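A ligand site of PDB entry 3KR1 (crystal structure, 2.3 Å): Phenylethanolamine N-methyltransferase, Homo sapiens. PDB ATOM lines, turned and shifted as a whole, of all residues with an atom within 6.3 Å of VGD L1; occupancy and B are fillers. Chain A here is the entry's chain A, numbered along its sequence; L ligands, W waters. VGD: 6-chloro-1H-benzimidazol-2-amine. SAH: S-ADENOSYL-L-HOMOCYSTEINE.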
ATOM      1  N   TYR A  35      -7.600 -20.070   5.980  1.00  0.00           N
ATOM      2  CA  TYR A  35      -8.264 -18.856   5.520  1.00  0.00           C
ATOM      3  C   TYR A  35      -7.241 -17.801   5.087  1.00  0.00           C
ATOM      4  O   TYR A  35      -7.371 -17.212   4.009  1.00  0.00           O
ATOM      5  CB  TYR A  35      -9.176 -18.278   6.611  1.00  0.00           C
ATOM      6  CG  TYR A  35      -9.876 -17.006   6.183  1.00  0.00           C
ATOM      7  CD1 TYR A  35     -10.922 -17.036   5.261  1.00  0.00           C
ATOM      8  CD2 TYR A  35      -9.500 -15.774   6.708  1.00  0.00           C
ATOM      9  CE1 TYR A  35     -11.559 -15.884   4.884  1.00  0.00           C
ATOM     10  CE2 TYR A  35     -10.128 -14.618   6.329  1.00  0.00           C
ATOM     11  CZ  TYR A  35     -11.163 -14.676   5.413  1.00  0.00           C
ATOM     12  OH  TYR A  35     -11.795 -13.511   5.032  1.00  0.00           O
ATOM     13  N   ASN A  39      -6.662 -16.429   1.053  1.00  0.00           N
ATOM     14  CA  ASN A  39      -7.121 -15.093   0.708  1.00  0.00           C
ATOM     15  C   ASN A  39      -6.073 -13.988   0.849  1.00  0.00           C
ATOM     16  O   ASN A  39      -6.229 -12.904   0.270  1.00  0.00           O
ATOM     17  CB  ASN A  39      -8.345 -14.748   1.546  1.00  0.00           C
ATOM     18  CG  ASN A  39      -9.534 -15.634   1.236  1.00  0.00           C
ATOM     19  OD1 ASN A  39     -10.049 -15.627   0.115  1.00  0.00           O
ATOM     20  ND2 ASN A  39      -9.984 -16.398   2.221  1.00  0.00           N
ATOM     21  N   TYR A  40      -5.031 -14.250   1.610  1.00  0.00           N
ATOM     22  CA  TYR A  40      -4.049 -13.205   1.916  1.00  0.00           C
ATOM     23  C   TYR A  40      -2.617 -13.627   1.640  1.00  0.00           C
ATOM     24  O   TYR A  40      -1.659 -12.991   2.083  1.00  0.00           O
ATOM     25  CB  TYR A  40      -4.254 -12.716   3.343  1.00  0.00           C
ATOM     26  CG  TYR A  40      -5.645 -12.154   3.521  1.00  0.00           C
ATOM     27  CD1 TYR A  40      -6.648 -12.899   4.119  1.00  0.00           C
ATOM     28  CD2 TYR A  40      -5.964 -10.900   3.024  1.00  0.00           C
ATOM     29  CE1 TYR A  40      -7.922 -12.387   4.254  1.00  0.00           C
ATOM     30  CE2 TYR A  40      -7.228 -10.385   3.158  1.00  0.00           C
ATOM     31  CZ  TYR A  40      -8.208 -11.129   3.773  1.00  0.00           C
ATOM     32  OH  TYR A  40      -9.470 -10.592   3.902  1.00  0.00           O
ATOM     33  N   ARG A  44      -3.696 -13.823  -4.406  1.00  0.00           N
ATOM     34  CA  ARG A  44      -4.527 -12.743  -3.890  1.00  0.00           C
ATOM     35  C   ARG A  44      -3.747 -11.802  -2.961  1.00  0.00           C
ATOM     36  O   ARG A  44      -4.087 -10.635  -2.817  1.00  0.00           O
ATOM     37  CB  ARG A  44      -5.757 -13.304  -3.176  1.00  0.00           C
ATOM     38  CG  ARG A  44      -6.776 -13.918  -4.133  1.00  0.00           C
ATOM     39  CD  ARG A  44      -8.063 -14.331  -3.446  1.00  0.00           C
ATOM     40  NE  ARG A  44      -8.976 -14.918  -4.420  1.00  0.00           N
ATOM     41  CZ  ARG A  44     -10.190 -15.390  -4.141  1.00  0.00           C
ATOM     42  NH1 ARG A  44     -10.659 -15.353  -2.902  1.00  0.00           N
ATOM     43  NH2 ARG A  44     -10.944 -15.904  -5.107  1.00  0.00           N
ATOM     44  N   VAL A  53      -6.768  -7.322  -5.958  1.00  0.00           N
ATOM     45  CA  VAL A  53      -7.825  -7.039  -4.980  1.00  0.00           C
ATOM     46  C   VAL A  53      -7.261  -6.402  -3.711  1.00  0.00           C
ATOM     47  O   VAL A  53      -7.910  -5.569  -3.086  1.00  0.00           O
ATOM     48  CB  VAL A  53      -8.609  -8.318  -4.615  1.00  0.00           C
ATOM     49  CG1 VAL A  53      -7.753  -9.256  -3.763  1.00  0.00           C
ATOM     50  CG2 VAL A  53      -9.903  -7.955  -3.887  1.00  0.00           C
ATOM     51  N   GLY A  54      -6.056  -6.813  -3.336  1.00  0.00           N
ATOM     52  CA  GLY A  54      -5.402  -6.317  -2.137  1.00  0.00           C
ATOM     53  C   GLY A  54      -5.180  -4.826  -2.179  1.00  0.00           C
ATOM     54  O   GLY A  54      -5.650  -4.095  -1.304  1.00  0.00           O
ATOM     55  N   LYS A  57      -8.523  -2.838  -2.154  1.00  0.00           N
ATOM     56  CA  LYS A  57      -9.109  -2.753  -0.821  1.00  0.00           C
ATOM     57  C   LYS A  57      -8.411  -1.702   0.051  1.00  0.00           C
ATOM     58  O   LYS A  57      -9.078  -0.893   0.703  1.00  0.00           O
ATOM     59  CB  LYS A  57      -9.080  -4.112  -0.114  1.00  0.00           C
ATOM     60  CG  LYS A  57     -10.198  -5.046  -0.534  1.00  0.00           C
ATOM     61  CD  LYS A  57     -10.290  -6.249   0.388  1.00  0.00           C
ATOM     62  CE  LYS A  57      -9.073  -7.154   0.245  1.00  0.00           C
ATOM     63  NZ  LYS A  57      -9.199  -8.361   1.099  1.00  0.00           N
ATOM     64  N   TYR A  85      -5.426  -6.170   8.256  1.00  0.00           N
ATOM     65  CA  TYR A  85      -5.243  -5.223   7.166  1.00  0.00           C
ATOM     66  C   TYR A  85      -6.332  -4.157   7.146  1.00  0.00           C
ATOM     67  O   TYR A  85      -6.073  -3.004   6.784  1.00  0.00           O
ATOM     68  CB  TYR A  85      -5.234  -5.936   5.821  1.00  0.00           C
ATOM     69  CG  TYR A  85      -6.605  -6.404   5.385  1.00  0.00           C
ATOM     70  CD1 TYR A  85      -7.411  -5.613   4.582  1.00  0.00           C
ATOM     71  CD2 TYR A  85      -7.098  -7.628   5.798  1.00  0.00           C
ATOM     72  CE1 TYR A  85      -8.663  -6.027   4.193  1.00  0.00           C
ATOM     73  CE2 TYR A  85      -8.343  -8.061   5.413  1.00  0.00           C
ATOM     74  CZ  TYR A  85      -9.120  -7.257   4.614  1.00  0.00           C
ATOM     75  OH  TYR A  85     -10.374  -7.693   4.230  1.00  0.00           O
ATOM     76  N   ALA A 181     -15.394  -6.397   7.377  1.00  0.00           N
ATOM     77  CA  ALA A 181     -15.003  -6.922   6.072  1.00  0.00           C
ATOM     78  C   ALA A 181     -15.257  -8.416   5.933  1.00  0.00           C
ATOM     79  O   ALA A 181     -14.741  -9.228   6.701  1.00  0.00           O
ATOM     80  CB  ALA A 181     -13.550  -6.606   5.802  1.00  0.00           C
ATOM     81  N   PHE A 182     -16.055  -8.769   4.924  1.00  0.00           N
ATOM     82  CA  PHE A 182     -16.348 -10.160   4.601  1.00  0.00           C
ATOM     83  C   PHE A 182     -16.980 -10.932   5.752  1.00  0.00           C
ATOM     84  O   PHE A 182     -16.771 -12.133   5.878  1.00  0.00           O
ATOM     85  CB  PHE A 182     -15.077 -10.896   4.145  1.00  0.00           C
ATOM     86  CG  PHE A 182     -14.415 -10.260   2.960  1.00  0.00           C
ATOM     87  CD1 PHE A 182     -13.275  -9.498   3.118  1.00  0.00           C
ATOM     88  CD2 PHE A 182     -14.937 -10.437   1.686  1.00  0.00           C
ATOM     89  CE1 PHE A 182     -12.652  -8.916   2.021  1.00  0.00           C
ATOM     90  CE2 PHE A 182     -14.320  -9.867   0.593  1.00  0.00           C
ATOM     91  CZ  PHE A 182     -13.179  -9.102   0.760  1.00  0.00           C
ATOM     92  N   ALA A 186     -21.034 -13.462   4.826  1.00  0.00           N
ATOM     93  CA  ALA A 186     -20.396 -14.749   5.069  1.00  0.00           C
ATOM     94  C   ALA A 186     -20.999 -15.525   6.249  1.00  0.00           C
ATOM     95  O   ALA A 186     -20.666 -16.694   6.467  1.00  0.00           O
ATOM     96  CB  ALA A 186     -18.887 -14.568   5.246  1.00  0.00           C
ATOM     97  N   ALA A 216     -17.839  -9.604  -0.168  1.00  0.00           N
ATOM     98  CA  ALA A 216     -17.862 -10.354  -1.408  1.00  0.00           C
ATOM     99  C   ALA A 216     -19.175 -10.103  -2.137  1.00  0.00           C
ATOM    100  O   ALA A 216     -20.234 -10.009  -1.528  1.00  0.00           O
ATOM    101  CB  ALA A 216     -17.707 -11.841  -1.129  1.00  0.00           C
ATOM    102  N   GLU A 219     -21.259 -14.113  -4.055  1.00  0.00           N
ATOM    103  CA  GLU A 219     -20.565 -15.312  -3.580  1.00  0.00           C
ATOM    104  C   GLU A 219     -21.538 -16.229  -2.854  1.00  0.00           C
ATOM    105  O   GLU A 219     -22.445 -15.753  -2.152  1.00  0.00           O
ATOM    106  CB  GLU A 219     -19.395 -14.930  -2.659  1.00  0.00           C
ATOM    107  CG  GLU A 219     -18.735 -16.119  -1.997  1.00  0.00           C
ATOM    108  CD  GLU A 219     -17.569 -15.710  -1.103  1.00  0.00           C
ATOM    109  OE1 GLU A 219     -16.501 -15.366  -1.647  1.00  0.00           O
ATOM    110  OE2 GLU A 219     -17.734 -15.740   0.139  1.00  0.00           O
ATOM    111  N   TYR A 222     -17.250 -20.431   0.355  1.00  0.00           N
ATOM    112  CA  TYR A 222     -15.801 -20.328   0.412  1.00  0.00           C
ATOM    113  C   TYR A 222     -15.255 -21.363   1.381  1.00  0.00           C
ATOM    114  O   TYR A 222     -15.967 -21.834   2.266  1.00  0.00           O
ATOM    115  CB  TYR A 222     -15.339 -18.908   0.772  1.00  0.00           C
ATOM    116  CG  TYR A 222     -15.554 -18.508   2.210  1.00  0.00           C
ATOM    117  CD1 TYR A 222     -14.489 -18.454   3.103  1.00  0.00           C
ATOM    118  CD2 TYR A 222     -16.816 -18.160   2.670  1.00  0.00           C
ATOM    119  CE1 TYR A 222     -14.680 -18.067   4.418  1.00  0.00           C
ATOM    120  CE2 TYR A 222     -17.017 -17.779   3.977  1.00  0.00           C
ATOM    121  CZ  TYR A 222     -15.942 -17.735   4.850  1.00  0.00           C
ATOM    122  OH  TYR A 222     -16.143 -17.354   6.157  1.00  0.00           O
ATOM    123  N   TYR A 256     -15.174  -3.825  -7.138  1.00  0.00           N
ATOM    124  CA  TYR A 256     -14.018  -4.404  -7.802  1.00  0.00           C
ATOM    125  C   TYR A 256     -14.450  -5.722  -8.437  1.00  0.00           C
ATOM    126  O   TYR A 256     -14.944  -6.612  -7.748  1.00  0.00           O
ATOM    127  CB  TYR A 256     -12.887  -4.643  -6.809  1.00  0.00           C
ATOM    128  CG  TYR A 256     -11.675  -5.373  -7.342  1.00  0.00           C
ATOM    129  CD1 TYR A 256     -10.658  -4.698  -7.997  1.00  0.00           C
ATOM    130  CD2 TYR A 256     -11.527  -6.740  -7.162  1.00  0.00           C
ATOM    131  CE1 TYR A 256      -9.534  -5.363  -8.473  1.00  0.00           C
ATOM    132  CE2 TYR A 256     -10.417  -7.419  -7.623  1.00  0.00           C
ATOM    133  CZ  TYR A 256      -9.419  -6.720  -8.281  1.00  0.00           C
ATOM    134  OH  TYR A 256      -8.314  -7.392  -8.754  1.00  0.00           O
ATOM    135  N   MET A 258     -13.686  -9.235  -9.971  1.00  0.00           N
ATOM    136  CA  MET A 258     -12.617 -10.210  -9.773  1.00  0.00           C
ATOM    137  C   MET A 258     -12.041 -10.689 -11.098  1.00  0.00           C
ATOM    138  O   MET A 258     -12.748 -11.286 -11.907  1.00  0.00           O
ATOM    139  CB  MET A 258     -13.134 -11.404  -8.972  1.00  0.00           C
ATOM    140  CG  MET A 258     -12.056 -12.229  -8.273  1.00  0.00           C
ATOM    141  SD  MET A 258     -11.186 -11.299  -7.001  1.00  0.00           S
ATOM    142  CE  MET A 258     -12.522 -10.303  -6.350  1.00  0.00           C
ATOM    143  N   LEU A 262      -7.445 -14.269 -10.291  1.00  0.00           N
ATOM    144  CA  LEU A 262      -7.653 -14.311  -8.846  1.00  0.00           C
ATOM    145  C   LEU A 262      -8.821 -15.224  -8.461  1.00  0.00           C
ATOM    146  O   LEU A 262      -9.220 -15.271  -7.293  1.00  0.00           O
ATOM    147  CB  LEU A 262      -7.826 -12.901  -8.270  1.00  0.00           C
ATOM    148  CG  LEU A 262      -6.609 -11.987  -8.279  1.00  0.00           C
ATOM    149  CD1 LEU A 262      -6.926 -10.671  -7.564  1.00  0.00           C
ATOM    150  CD2 LEU A 262      -5.386 -12.650  -7.653  1.00  0.00           C
ATOM    151  N   ASP A 267     -13.212 -20.221  -3.481  1.00  0.00           N
ATOM    152  CA  ASP A 267     -14.567 -19.682  -3.384  1.00  0.00           C
ATOM    153  C   ASP A 267     -15.093 -19.394  -4.785  1.00  0.00           C
ATOM    154  O   ASP A 267     -14.451 -19.731  -5.778  1.00  0.00           O
ATOM    155  CB  ASP A 267     -14.594 -18.433  -2.510  1.00  0.00           C
ATOM    156  CG  ASP A 267     -13.682 -17.328  -3.034  1.00  0.00           C
ATOM    157  OD1 ASP A 267     -13.640 -17.127  -4.270  1.00  0.00           O
ATOM    158  OD2 ASP A 267     -13.020 -16.661  -2.216  1.00  0.00           O
ATOM    159  N   VAL A 269     -16.368 -16.110  -5.483  1.00  0.00           N
ATOM    160  CA  VAL A 269     -16.584 -14.670  -5.425  1.00  0.00           C
ATOM    161  C   VAL A 269     -16.515 -14.055  -6.830  1.00  0.00           C
ATOM    162  O   VAL A 269     -15.672 -14.432  -7.630  1.00  0.00           O
ATOM    163  CB  VAL A 269     -15.562 -13.984  -4.495  1.00  0.00           C
ATOM    164  CG1 VAL A 269     -14.157 -14.192  -5.023  1.00  0.00           C
ATOM    165  CG2 VAL A 269     -15.872 -12.513  -4.362  1.00  0.00           C
ATOM    166  N   GLY A 271     -16.945 -10.479  -7.243  1.00  0.00           N
ATOM    167  CA  GLY A 271     -16.419  -9.138  -7.088  1.00  0.00           C
ATOM    168  C   GLY A 271     -16.279  -8.812  -5.620  1.00  0.00           C
ATOM    169  O   GLY A 271     -16.616  -9.634  -4.769  1.00  0.00           O
ATOM    170  N   VAL A 272     -15.778  -7.629  -5.324  1.00  0.00           N
ATOM    171  CA  VAL A 272     -15.665  -7.159  -3.958  1.00  0.00           C
ATOM    172  C   VAL A 272     -16.264  -5.759  -3.901  1.00  0.00           C
ATOM    173  O   VAL A 272     -16.007  -4.942  -4.784  1.00  0.00           O
ATOM    174  CB  VAL A 272     -14.198  -7.123  -3.476  1.00  0.00           C
ATOM    175  CG1 VAL A 272     -14.109  -6.487  -2.103  1.00  0.00           C
ATOM    176  CG2 VAL A 272     -13.624  -8.530  -3.456  1.00  0.00           C
HETATM  177 CLA  VGD L   1     -10.803 -11.675  -4.008  1.00  0.00          CL
HETATM  178  CAH VGD L   1     -10.936 -11.859  -2.251  1.00  0.00           C
HETATM  179  CAC VGD L   1      -9.952 -11.337  -1.424  1.00  0.00           C
HETATM  180  CAD VGD L   1     -10.032 -11.472  -0.045  1.00  0.00           C
HETATM  181  CAK VGD L   1     -11.122 -12.151   0.506  1.00  0.00           C
HETATM  182  CAJ VGD L   1     -12.112 -12.685  -0.318  1.00  0.00           C
HETATM  183  CAE VGD L   1     -12.008 -12.533  -1.714  1.00  0.00           C
HETATM  184  NAG VGD L   1     -11.484 -12.440   1.817  1.00  0.00           N
HETATM  185  CAI VGD L   1     -12.662 -13.135   1.813  1.00  0.00           C
HETATM  186  NAF VGD L   1     -13.057 -13.289   0.509  1.00  0.00           N
HETATM  187  NAA VGD L   1     -13.339 -13.617   2.975  1.00  0.00           N
HETATM  188  N   SAH L   2     -12.673  -9.637   8.466  1.00  0.00           N
HETATM  189  CA  SAH L   2     -11.771 -10.665   7.962  1.00  0.00           C
HETATM  190  CB  SAH L   2     -12.319 -12.074   8.196  1.00  0.00           C
HETATM  191  CG  SAH L   2     -13.619 -12.388   7.449  1.00  0.00           C
HETATM  192  SD  SAH L   2     -14.033 -14.161   7.546  1.00  0.00           S
HETATM  193  C   SAH L   2     -11.432 -10.393   6.492  1.00  0.00           C
HETATM  194  O   SAH L   2     -10.790 -11.223   5.951  1.00  0.00           O
HETATM  195  OXT SAH L   2     -11.517  -9.054   6.085  1.00  0.00           O
HETATM  196  C5' SAH L   2     -15.668 -14.101   8.348  1.00  0.00           C
HETATM  197  C4' SAH L   2     -15.642 -14.091   9.880  1.00  0.00           C
HETATM  198  O4' SAH L   2     -16.940 -14.189  10.352  1.00  0.00           O
HETATM  199  C3' SAH L   2     -14.967 -15.331  10.469  1.00  0.00           C
HETATM  200  O3' SAH L   2     -13.828 -14.912  11.179  1.00  0.00           O
HETATM  201  C2' SAH L   2     -15.911 -15.864  11.321  1.00  0.00           C
HETATM  202  O2' SAH L   2     -15.360 -16.368  12.509  1.00  0.00           O
HETATM  203  C1' SAH L   2     -16.792 -14.773  11.592  1.00  0.00           C
HETATM  204  N9  SAH L   2     -18.092 -15.181  12.104  1.00  0.00           N
HETATM  205  C8  SAH L   2     -18.684 -16.361  11.961  1.00  0.00           C
HETATM  206  N7  SAH L   2     -19.926 -16.306  12.557  1.00  0.00           N
HETATM  207  C5  SAH L   2     -20.075 -15.048  13.083  1.00  0.00           C
HETATM  208  C6  SAH L   2     -21.101 -14.458  13.771  1.00  0.00           C
HETATM  209  N6  SAH L   2     -22.301 -15.203  14.070  1.00  0.00           N
HETATM  210  N1  SAH L   2     -20.993 -13.199  14.176  1.00  0.00           N
HETATM  211  C2  SAH L   2     -19.874 -12.493  13.894  1.00  0.00           C
HETATM  212  N3  SAH L   2     -18.861 -13.077  13.206  1.00  0.00           N
HETATM  213  C4  SAH L   2     -18.974 -14.348  12.805  1.00  0.00           C
HETATM  214  O   HOH W   1     -15.164 -14.906   1.341  1.00  0.00           O
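The side-chain hydroxyl (OH) of Tyr 40 is in hydrogen-bond range of an oxygen (O) of SAH L2, at 2.5 Å. NAA of VGD L1 sits at hydrogen-bond distance from OH of Tyr 35 (2.6 Å). The backbone carbonyl oxygen (O) of Ala 181 lies within hydrogen-bond range of a nitrogen (N) of SAH L2 (2.7 Å). OH of Tyr 85 is in hydrogen-bond range of OXT of SAH L2 (2.6 Å). An oxygen (O) of SAH L2 is in hydrogen-bond range of the side-chain hydroxyl (OH) of Tyr 35 (2.7 Å). A nitrogen (NAG) of VGD L1 sits at hydrogen-bond distance from the side-chain hydroxyl of Tyr 40, at 3.4 Å.
The side-chain hydroxyl (OH) of Tyr 40 is in hydrogen-bond range of the side-chain hydroxyl (OH) of Tyr 85 (3.1 Å). The side-chain hydroxyl of Tyr 85 sits at hydrogen-bond distance from the side-chain amino group of Lys 57 (3.4 Å). OH of Tyr 256 is in hydrogen-bond range of N of Val 53, 3.2 Å away. The side-chain amide nitrogen of Asn 39 sits close to the backbone carbonyl oxygen of Tyr 35 (3.3 Å). The guanidinium group of Arg 44 lies within hydrogen-bond range of the backbone carbonyl oxygen of Leu 262 (2.9 Å). OD1 of Asn 39 is in hydrogen-bond range of NH1 of Arg 44, 3.1 Å away. The guanidinium group of Arg 44 lies within salt-bridge range of the side-chain carboxylate of Asp 267 (2.8 Å).
Asn 39 touches VGD L1. Arg 44 touches VGD L1 (NH1 to CAE, 3.3 Å). Val 53 touches VGD L1 (CG1 to CAC, 3.8 Å). NZ of Lys 57 touches CAD of VGD L1, at 3.4 Å. CB of Phe 182 touches NAA of VGD L1, at 3.4 Å. Met 258 touches VGD L1 (SD to CLA, 3.0 Å). Hydrophobic or aromatic side chains within 4 Å of VGD L1: Tyr 35, Val 53, Phe 182 and Met 258. The nearest printed residue that does not touch VGD L1 is Val 272 (4.3 Å).
Water W1 lies within hydrogen-bond range of a nitrogen (NAA) of VGD L1 and the side-chain carboxylate (OE2) of Glu 219.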
